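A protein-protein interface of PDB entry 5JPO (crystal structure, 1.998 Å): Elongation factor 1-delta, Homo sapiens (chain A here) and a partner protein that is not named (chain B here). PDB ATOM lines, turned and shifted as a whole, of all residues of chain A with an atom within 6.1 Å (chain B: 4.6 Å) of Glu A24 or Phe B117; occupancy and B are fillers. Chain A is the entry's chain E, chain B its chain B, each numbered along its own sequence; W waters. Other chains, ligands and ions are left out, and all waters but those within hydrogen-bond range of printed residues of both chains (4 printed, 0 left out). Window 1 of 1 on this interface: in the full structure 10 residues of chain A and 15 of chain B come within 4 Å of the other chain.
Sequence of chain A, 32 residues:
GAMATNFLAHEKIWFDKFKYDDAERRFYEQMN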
ATOM      1  N   LYS A  19      -6.939  17.343 -19.669  1.00  0.00           N
ATOM      2  CA  LYS A  19      -5.942  18.200 -20.318  1.00  0.00           C
ATOM      3  C   LYS A  19      -5.249  17.450 -21.454  1.00  0.00           C
ATOM      4  O   LYS A  19      -5.042  17.986 -22.545  1.00  0.00           O
ATOM      5  CB  LYS A  19      -4.894  18.704 -19.315  1.00  0.00           C
ATOM      6  CG  LYS A  19      -5.428  19.676 -18.265  1.00  0.00           C
ATOM      7  CD  LYS A  19      -4.348  20.034 -17.247  1.00  0.00           C
ATOM      8  CE  LYS A  19      -4.949  20.516 -15.919  1.00  0.00           C
ATOM      9  NZ  LYS A  19      -3.905  20.802 -14.872  1.00  0.00           N
ATOM     10  N   TYR A  20      -4.889  16.204 -21.176  1.00  0.00           N
ATOM     11  CA  TYR A  20      -4.244  15.347 -22.159  1.00  0.00           C
ATOM     12  C   TYR A  20      -5.176  14.996 -23.318  1.00  0.00           C
ATOM     13  O   TYR A  20      -4.779  15.098 -24.473  1.00  0.00           O
ATOM     14  CB  TYR A  20      -3.725  14.083 -21.473  1.00  0.00           C
ATOM     15  CG  TYR A  20      -2.446  14.365 -20.743  1.00  0.00           C
ATOM     16  CD1 TYR A  20      -1.217  14.104 -21.343  1.00  0.00           C
ATOM     17  CD2 TYR A  20      -2.455  14.938 -19.484  1.00  0.00           C
ATOM     18  CE1 TYR A  20      -0.038  14.379 -20.706  1.00  0.00           C
ATOM     19  CE2 TYR A  20      -1.269  15.218 -18.826  1.00  0.00           C
ATOM     20  CZ  TYR A  20      -0.062  14.939 -19.450  1.00  0.00           C
ATOM     21  OH  TYR A  20       1.128  15.211 -18.822  1.00  0.00           O
ATOM     22  N   ASP A  21      -6.406  14.592 -23.013  1.00  0.00           N
ATOM     23  CA  ASP A  21      -7.372  14.271 -24.052  1.00  0.00           C
ATOM     24  C   ASP A  21      -7.650  15.480 -24.940  1.00  0.00           C
ATOM     25  O   ASP A  21      -7.831  15.344 -26.147  1.00  0.00           O
ATOM     26  CB  ASP A  21      -8.681  13.760 -23.439  1.00  0.00           C
ATOM     27  CG  ASP A  21      -8.572  12.340 -22.940  1.00  0.00           C
ATOM     28  OD1 ASP A  21      -7.509  11.710 -23.155  1.00  0.00           O
ATOM     29  OD2 ASP A  21      -9.556  11.845 -22.347  1.00  0.00           O
ATOM     30  N   ASP A  22      -7.666  16.666 -24.346  1.00  0.00           N
ATOM     31  CA  ASP A  22      -7.956  17.871 -25.114  1.00  0.00           C
ATOM     32  C   ASP A  22      -6.791  18.265 -26.028  1.00  0.00           C
ATOM     33  O   ASP A  22      -7.004  18.648 -27.182  1.00  0.00           O
ATOM     34  CB  ASP A  22      -8.310  19.032 -24.185  1.00  0.00           C
ATOM     35  CG  ASP A  22      -8.635  20.290 -24.947  1.00  0.00           C
ATOM     36  OD1 ASP A  22      -9.785  20.404 -25.411  1.00  0.00           O
ATOM     37  OD2 ASP A  22      -7.733  21.142 -25.104  1.00  0.00           O
ATOM     38  N   ALA A  23      -5.566  18.163 -25.515  1.00  0.00           N
ATOM     39  CA  ALA A  23      -4.372  18.445 -26.316  1.00  0.00           C
ATOM     40  C   ALA A  23      -4.241  17.454 -27.472  1.00  0.00           C
ATOM     41  O   ALA A  23      -3.883  17.832 -28.585  1.00  0.00           O
ATOM     42  CB  ALA A  23      -3.116  18.410 -25.442  1.00  0.00           C
ATOM     43  N   GLU A  24      -4.538  16.191 -27.192  1.00  0.00           N
ATOM     44  CA  GLU A  24      -4.426  15.125 -28.179  1.00  0.00           C
ATOM     45  C   GLU A  24      -5.458  15.317 -29.290  1.00  0.00           C
ATOM     46  O   GLU A  24      -5.120  15.232 -30.472  1.00  0.00           O
ATOM     47  CB  GLU A  24      -4.592  13.749 -27.515  1.00  0.00           C
ATOM     48  CG  GLU A  24      -4.550  12.572 -28.500  1.00  0.00           C
ATOM     49  CD  GLU A  24      -4.550  11.206 -27.818  1.00  0.00           C
ATOM     50  OE1 GLU A  24      -5.307  10.999 -26.844  1.00  0.00           O
ATOM     51  OE2 GLU A  24      -3.788  10.331 -28.269  1.00  0.00           O
ATOM     52  N   ARG A  25      -6.706  15.579 -28.908  1.00  0.00           N
ATOM     53  CA  ARG A  25      -7.766  15.866 -29.872  1.00  0.00           C
ATOM     54  C   ARG A  25      -7.344  16.997 -30.812  1.00  0.00           C
ATOM     55  O   ARG A  25      -7.404  16.865 -32.034  1.00  0.00           O
ATOM     56  CB  ARG A  25      -9.071  16.235 -29.152  1.00  0.00           C
ATOM     57  CG  ARG A  25     -10.171  16.712 -30.089  1.00  0.00           C
ATOM     58  CD  ARG A  25     -11.432  17.196 -29.337  1.00  0.00           C
ATOM     59  NE  ARG A  25     -11.180  18.365 -28.488  1.00  0.00           N
ATOM     60  CZ  ARG A  25     -11.089  19.615 -28.936  1.00  0.00           C
ATOM     61  NH1 ARG A  25     -11.222  19.876 -30.229  1.00  0.00           N
ATOM     62  NH2 ARG A  25     -10.855  20.607 -28.089  1.00  0.00           N
ATOM     63  N   ARG A  26      -6.902  18.102 -30.224  1.00  0.00           N
ATOM     64  CA  ARG A  26      -6.468  19.266 -30.988  1.00  0.00           C
ATOM     65  C   ARG A  26      -5.330  18.931 -31.930  1.00  0.00           C
ATOM     66  O   ARG A  26      -5.309  19.398 -33.063  1.00  0.00           O
ATOM     67  CB  ARG A  26      -6.035  20.398 -30.051  1.00  0.00           C
ATOM     68  CG  ARG A  26      -7.193  21.097 -29.360  1.00  0.00           C
ATOM     69  CD  ARG A  26      -6.706  22.123 -28.350  1.00  0.00           C
ATOM     70  NE  ARG A  26      -7.820  22.740 -27.631  1.00  0.00           N
ATOM     71  CZ  ARG A  26      -8.436  23.855 -28.016  1.00  0.00           C
ATOM     72  NH1 ARG A  26      -8.038  24.491 -29.112  1.00  0.00           N
ATOM     73  NH2 ARG A  26      -9.445  24.338 -27.297  1.00  0.00           N
ATOM     74  N   PHE A  27      -4.387  18.121 -31.454  1.00  0.00           N
ATOM     75  CA  PHE A  27      -3.224  17.732 -32.245  1.00  0.00           C
ATOM     76  C   PHE A  27      -3.645  17.019 -33.528  1.00  0.00           C
ATOM     77  O   PHE A  27      -3.191  17.364 -34.617  1.00  0.00           O
ATOM     78  CB  PHE A  27      -2.303  16.843 -31.405  1.00  0.00           C
ATOM     79  CG  PHE A  27      -1.084  16.347 -32.132  1.00  0.00           C
ATOM     80  CD1 PHE A  27       0.040  17.156 -32.269  1.00  0.00           C
ATOM     81  CD2 PHE A  27      -1.044  15.055 -32.640  1.00  0.00           C
ATOM     82  CE1 PHE A  27       1.170  16.697 -32.918  1.00  0.00           C
ATOM     83  CE2 PHE A  27       0.083  14.587 -33.288  1.00  0.00           C
ATOM     84  CZ  PHE A  27       1.193  15.412 -33.432  1.00  0.00           C
ATOM     85  N   TYR A  28      -4.522  16.030 -33.406  1.00  0.00           N
ATOM     86  CA  TYR A  28      -4.919  15.255 -34.577  1.00  0.00           C
ATOM     87  C   TYR A  28      -5.924  15.997 -35.465  1.00  0.00           C
ATOM     88  O   TYR A  28      -5.951  15.788 -36.674  1.00  0.00           O
ATOM     89  CB  TYR A  28      -5.469  13.895 -34.144  1.00  0.00           C
ATOM     90  CG  TYR A  28      -4.366  12.997 -33.638  1.00  0.00           C
ATOM     91  CD1 TYR A  28      -3.447  12.438 -34.522  1.00  0.00           C
ATOM     92  CD2 TYR A  28      -4.213  12.736 -32.279  1.00  0.00           C
ATOM     93  CE1 TYR A  28      -2.417  11.633 -34.074  1.00  0.00           C
ATOM     94  CE2 TYR A  28      -3.171  11.923 -31.819  1.00  0.00           C
ATOM     95  CZ  TYR A  28      -2.281  11.380 -32.726  1.00  0.00           C
ATOM     96  OH  TYR A  28      -1.255  10.574 -32.297  1.00  0.00           O
ATOM     97  N   GLU A  29      -6.726  16.881 -34.882  1.00  0.00           N
ATOM     98  CA  GLU A  29      -7.641  17.698 -35.688  1.00  0.00           C
ATOM     99  C   GLU A  29      -6.873  18.623 -36.635  1.00  0.00           C
ATOM    100  O   GLU A  29      -7.312  18.862 -37.760  1.00  0.00           O
ATOM    101  CB  GLU A  29      -8.572  18.530 -34.801  1.00  0.00           C
ATOM    102  CG  GLU A  29      -9.662  17.735 -34.109  1.00  0.00           C
ATOM    103  CD  GLU A  29     -10.623  18.611 -33.311  1.00  0.00           C
ATOM    104  OE1 GLU A  29     -10.379  19.832 -33.227  1.00  0.00           O
ATOM    105  OE2 GLU A  29     -11.630  18.081 -32.784  1.00  0.00           O
ATOM    106  N   TYR B  11      -8.857   8.846 -36.643  1.00  0.00           N
ATOM    107  CA  TYR B  11      -7.756   9.498 -37.331  1.00  0.00           C
ATOM    108  C   TYR B  11      -6.665   8.447 -37.521  1.00  0.00           C
ATOM    109  O   TYR B  11      -6.693   7.394 -36.871  1.00  0.00           O
ATOM    110  CB  TYR B  11      -7.240  10.723 -36.561  1.00  0.00           C
ATOM    111  CG  TYR B  11      -7.005  10.499 -35.082  1.00  0.00           C
ATOM    112  CD1 TYR B  11      -5.819   9.928 -34.621  1.00  0.00           C
ATOM    113  CD2 TYR B  11      -7.960  10.879 -34.147  1.00  0.00           C
ATOM    114  CE1 TYR B  11      -5.607   9.725 -33.267  1.00  0.00           C
ATOM    115  CE2 TYR B  11      -7.761  10.680 -32.800  1.00  0.00           C
ATOM    116  CZ  TYR B  11      -6.582  10.104 -32.362  1.00  0.00           C
ATOM    117  OH  TYR B  11      -6.394   9.919 -31.014  1.00  0.00           O
ATOM    118  N   ARG B  16      -5.263   3.310 -30.195  1.00  0.00           N
ATOM    119  CA  ARG B  16      -6.567   2.823 -29.771  1.00  0.00           C
ATOM    120  C   ARG B  16      -7.265   2.066 -30.896  1.00  0.00           C
ATOM    121  O   ARG B  16      -7.950   1.064 -30.658  1.00  0.00           O
ATOM    122  CB  ARG B  16      -7.443   3.980 -29.296  1.00  0.00           C
ATOM    123  CG  ARG B  16      -6.953   4.642 -28.021  1.00  0.00           C
ATOM    124  CD  ARG B  16      -7.960   5.691 -27.542  1.00  0.00           C
ATOM    125  NE  ARG B  16      -7.352   6.614 -26.592  1.00  0.00           N
ATOM    126  CZ  ARG B  16      -6.591   7.646 -26.946  1.00  0.00           C
ATOM    127  NH1 ARG B  16      -6.331   7.872 -28.229  1.00  0.00           N
ATOM    128  NH2 ARG B  16      -6.072   8.441 -26.019  1.00  0.00           N
ATOM    129  N   SER B 113       1.387   8.589 -21.441  1.00  0.00           N
ATOM    130  CA  SER B 113       0.997   9.828 -22.107  1.00  0.00           C
ATOM    131  C   SER B 113       1.869  10.970 -21.610  1.00  0.00           C
ATOM    132  O   SER B 113       2.353  11.782 -22.394  1.00  0.00           O
ATOM    133  CB  SER B 113      -0.492  10.145 -21.864  1.00  0.00           C
ATOM    134  OG  SER B 113      -1.335   9.129 -22.409  1.00  0.00           O
ATOM    135  N   THR B 114       2.079  11.017 -20.301  1.00  0.00           N
ATOM    136  CA  THR B 114       2.795  12.135 -19.705  1.00  0.00           C
ATOM    137  C   THR B 114       4.207  12.202 -20.256  1.00  0.00           C
ATOM    138  O   THR B 114       4.708  13.269 -20.605  1.00  0.00           O
ATOM    139  CB  THR B 114       2.826  12.020 -18.184  1.00  0.00           C
ATOM    140  OG1 THR B 114       1.482  12.041 -17.687  1.00  0.00           O
ATOM    141  CG2 THR B 114       3.606  13.180 -17.570  1.00  0.00           C
ATOM    142  N   TRP B 115       4.838  11.043 -20.377  1.00  0.00           N
ATOM    143  CA  TRP B 115       6.191  10.995 -20.866  1.00  0.00           C
ATOM    144  C   TRP B 115       6.246  11.241 -22.382  1.00  0.00           C
ATOM    145  O   TRP B 115       7.083  11.992 -22.875  1.00  0.00           O
ATOM    146  CB  TRP B 115       6.805   9.640 -20.504  1.00  0.00           C
ATOM    147  CG  TRP B 115       8.286   9.542 -20.715  1.00  0.00           C
ATOM    148  CD1 TRP B 115       9.109  10.495 -21.240  1.00  0.00           C
ATOM    149  CD2 TRP B 115       9.115   8.412 -20.408  1.00  0.00           C
ATOM    150  NE1 TRP B 115      10.413  10.031 -21.263  1.00  0.00           N
ATOM    151  CE2 TRP B 115      10.443   8.758 -20.766  1.00  0.00           C
ATOM    152  CE3 TRP B 115       8.872   7.153 -19.861  1.00  0.00           C
ATOM    153  CZ2 TRP B 115      11.520   7.872 -20.608  1.00  0.00           C
ATOM    154  CZ3 TRP B 115       9.952   6.267 -19.701  1.00  0.00           C
ATOM    155  CH2 TRP B 115      11.257   6.642 -20.070  1.00  0.00           C
ATOM    156  N   VAL B 116       5.349  10.624 -23.128  1.00  0.00           N
ATOM    157  CA  VAL B 116       5.476  10.646 -24.582  1.00  0.00           C
ATOM    158  C   VAL B 116       4.966  11.930 -25.251  1.00  0.00           C
ATOM    159  O   VAL B 116       5.577  12.411 -26.207  1.00  0.00           O
ATOM    160  CB  VAL B 116       4.749   9.427 -25.191  1.00  0.00           C
ATOM    161  CG1 VAL B 116       4.546   9.586 -26.685  1.00  0.00           C
ATOM    162  CG2 VAL B 116       5.535   8.145 -24.881  1.00  0.00           C
ATOM    163  N   PHE B 117       3.862  12.490 -24.762  1.00  0.00           N
ATOM    164  CA  PHE B 117       3.229  13.629 -25.458  1.00  0.00           C
ATOM    165  C   PHE B 117       4.187  14.812 -25.735  1.00  0.00           C
ATOM    166  O   PHE B 117       4.135  15.386 -26.825  1.00  0.00           O
ATOM    167  CB  PHE B 117       1.996  14.125 -24.690  1.00  0.00           C
ATOM    168  CG  PHE B 117       0.737  13.325 -24.964  1.00  0.00           C
ATOM    169  CD1 PHE B 117       0.810  12.017 -25.438  1.00  0.00           C
ATOM    170  CD2 PHE B 117      -0.515  13.885 -24.760  1.00  0.00           C
ATOM    171  CE1 PHE B 117      -0.342  11.285 -25.689  1.00  0.00           C
ATOM    172  CE2 PHE B 117      -1.671  13.161 -25.012  1.00  0.00           C
ATOM    173  CZ  PHE B 117      -1.584  11.858 -25.476  1.00  0.00           C
ATOM    174  N   PRO B 118       5.073  15.174 -24.779  1.00  0.00           N
ATOM    175  CA  PRO B 118       6.001  16.249 -25.153  1.00  0.00           C
ATOM    176  C   PRO B 118       6.918  15.893 -26.324  1.00  0.00           C
ATOM    177  O   PRO B 118       7.217  16.773 -27.129  1.00  0.00           O
ATOM    178  CB  PRO B 118       6.818  16.456 -23.881  1.00  0.00           C
ATOM    179  CG  PRO B 118       5.865  16.091 -22.782  1.00  0.00           C
ATOM    180  CD  PRO B 118       5.157  14.876 -23.336  1.00  0.00           C
ATOM    181  N   THR B 119       7.339  14.633 -26.428  1.00  0.00           N
ATOM    182  CA  THR B 119       8.245  14.234 -27.502  1.00  0.00           C
ATOM    183  C   THR B 119       7.557  14.272 -28.860  1.00  0.00           C
ATOM    184  O   THR B 119       8.219  14.274 -29.900  1.00  0.00           O
ATOM    185  CB  THR B 119       8.811  12.817 -27.285  1.00  0.00           C
ATOM    186  OG1 THR B 119       7.777  11.852 -27.524  1.00  0.00           O
ATOM    187  CG2 THR B 119       9.335  12.672 -25.870  1.00  0.00           C
ATOM    188  N   LEU B 120       6.229  14.299 -28.848  1.00  0.00           N
ATOM    189  CA  LEU B 120       5.465  14.336 -30.084  1.00  0.00           C
ATOM    190  C   LEU B 120       4.953  15.738 -30.394  1.00  0.00           C
ATOM    191  O   LEU B 120       4.319  15.954 -31.424  1.00  0.00           O
ATOM    192  CB  LEU B 120       4.283  13.362 -30.023  1.00  0.00           C
ATOM    193  CG  LEU B 120       4.591  11.868 -30.002  1.00  0.00           C
ATOM    194  CD1 LEU B 120       3.301  11.097 -29.812  1.00  0.00           C
ATOM    195  CD2 LEU B 120       5.300  11.431 -31.281  1.00  0.00           C
ATOM    196  N   GLY B 121       5.229  16.688 -29.511  1.00  0.00           N
ATOM    197  CA  GLY B 121       4.738  18.044 -29.691  1.00  0.00           C
ATOM    198  C   GLY B 121       3.250  18.211 -29.401  1.00  0.00           C
ATOM    199  O   GLY B 121       2.616  19.161 -29.864  1.00  0.00           O
ATOM    200  N   ILE B 122       2.681  17.290 -28.629  1.00  0.00           N
ATOM    201  CA  ILE B 122       1.272  17.388 -28.249  1.00  0.00           C
ATOM    202  C   ILE B 122       1.099  18.249 -27.003  1.00  0.00           C
ATOM    203  O   ILE B 122       0.112  18.985 -26.885  1.00  0.00           O
ATOM    204  CB  ILE B 122       0.654  15.995 -28.007  1.00  0.00           C
ATOM    205  CG1 ILE B 122       0.841  15.119 -29.250  1.00  0.00           C
ATOM    206  CG2 ILE B 122      -0.833  16.117 -27.645  1.00  0.00           C
ATOM    207  CD1 ILE B 122       0.232  13.723 -29.133  1.00  0.00           C
ATOM    208  N   MET B 123       2.056  18.161 -26.078  1.00  0.00           N
ATOM    209  CA  MET B 123       2.019  18.941 -24.834  1.00  0.00           C
ATOM    210  C   MET B 123       3.350  19.632 -24.604  1.00  0.00           C
ATOM    211  O   MET B 123       4.382  19.138 -25.043  1.00  0.00           O
ATOM    212  CB  MET B 123       1.722  18.056 -23.617  1.00  0.00           C
ATOM    213  CG  MET B 123       0.395  17.355 -23.618  1.00  0.00           C
ATOM    214  SD  MET B 123      -0.835  18.233 -22.633  1.00  0.00           S
ATOM    215  CE  MET B 123       0.085  18.483 -21.125  1.00  0.00           C
HETATM  216  O   HOH W   1      -4.041   8.291 -30.426  1.00  0.00           O
HETATM  217  O   HOH W   2       3.409  15.684 -20.588  1.00  0.00           O
HETATM  218  O   HOH W   3      -2.056  19.660 -28.662  1.00  0.00           O
HETATM  219  O   HOH W   4      -2.952   8.616 -26.357  1.00  0.00           O
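Printed residues of chain B that touch a printed residue of chain A: Tyr B11, Arg B16, Ser B113, Thr B114, Phe B117, Leu B120, Ile B122 and Met B123. Hydrophobic or aromatic side chains of chain B within 4 Å of the printed part of chain A: Tyr B11, Phe B117, Ile B122 and Met B123. Printed residues of chain A that touch a printed residue of chain B: Tyr A20, Ala A23, Glu A24, Phe A27 and Tyr A28. Hydrophobic or aromatic side chains of chain A within 4 Å of the printed part of chain B: Tyr A20, Ala A23, Phe A27 and Tyr A28. Among the printed residues, 13 pairs touch across the chains.
Water W3 bridges O of Ala A23 (2.6 Å) and O of Ile B122 (2.9 Å). Water W4 bridges the side-chain carboxylate of Glu A24 (2.7 Å) and the guanidinium group of Arg B16 (3.1 Å). Water W2 bridges O of Thr B114 (2.7 Å) and OH of Tyr A20 (2.9 Å). Water W1 lies within hydrogen-bond range of OH of Tyr B11 (2.9 Å), OE2 of Glu A24 (3.0 Å) and NH1 of Arg B16 (3.2 Å).
Of chain B, only Tyr B11, Arg B16, Phe B117 and Ile B122 come within 4 Å of Glu A24. Phe B117 touches just these residues of chain A: Tyr A20 (3.5 Å) and Glu A24 (3.8 Å). Of the printed residues of chain B, Ala A23 touches Ile B122 and Met B123. Of the printed residues of chain B, Phe A27 touches Leu B120 (3.6 Å) and Ile B122 (3.7 Å). Printed residues of chain A within 4 Å of Tyr B11: Glu A24 (3.8 Å) and Tyr A28 (3.5 Å). Asp A21 touches none of the printed residues of chain B. Trp B115 touches none of the printed residues of chain A. The nearest printed residue of chain B that does not touch Glu A24 is Met B123 (6.2 Å). The nearest residue of chain A that does not touch Phe B117 is Ala A23 (5.3 Å).
Among the printed residues, pairs that only touch across the chains: Tyr A28 with Tyr B11, Tyr A20 with Phe B117, Phe A27 with Leu B120, Ala A23 with Ile B122, Ala A23 with Met B123, Phe A27 with Ile B122, Glu A24 with Ile B122, Glu A24 with Tyr B11, Glu A24 with Phe B117, Tyr A20 with Ser B113 and Tyr A20 with Met B123.
The side-chain hydroxyl (OH) of Tyr B11 lies within hydrogen-bond range of the guanidinium group (NH1) of Arg B16. O of Phe B117 sits at hydrogen-bond distance from N of Ile B122 (3.0 Å).
OG1 of Thr B114 lies within hydrogen-bond range of OH of Tyr A20 (3.4 Å). The side-chain carboxylate of Glu A24 is in salt-bridge range of the guanidinium group of Arg B16 (2.8 Å).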
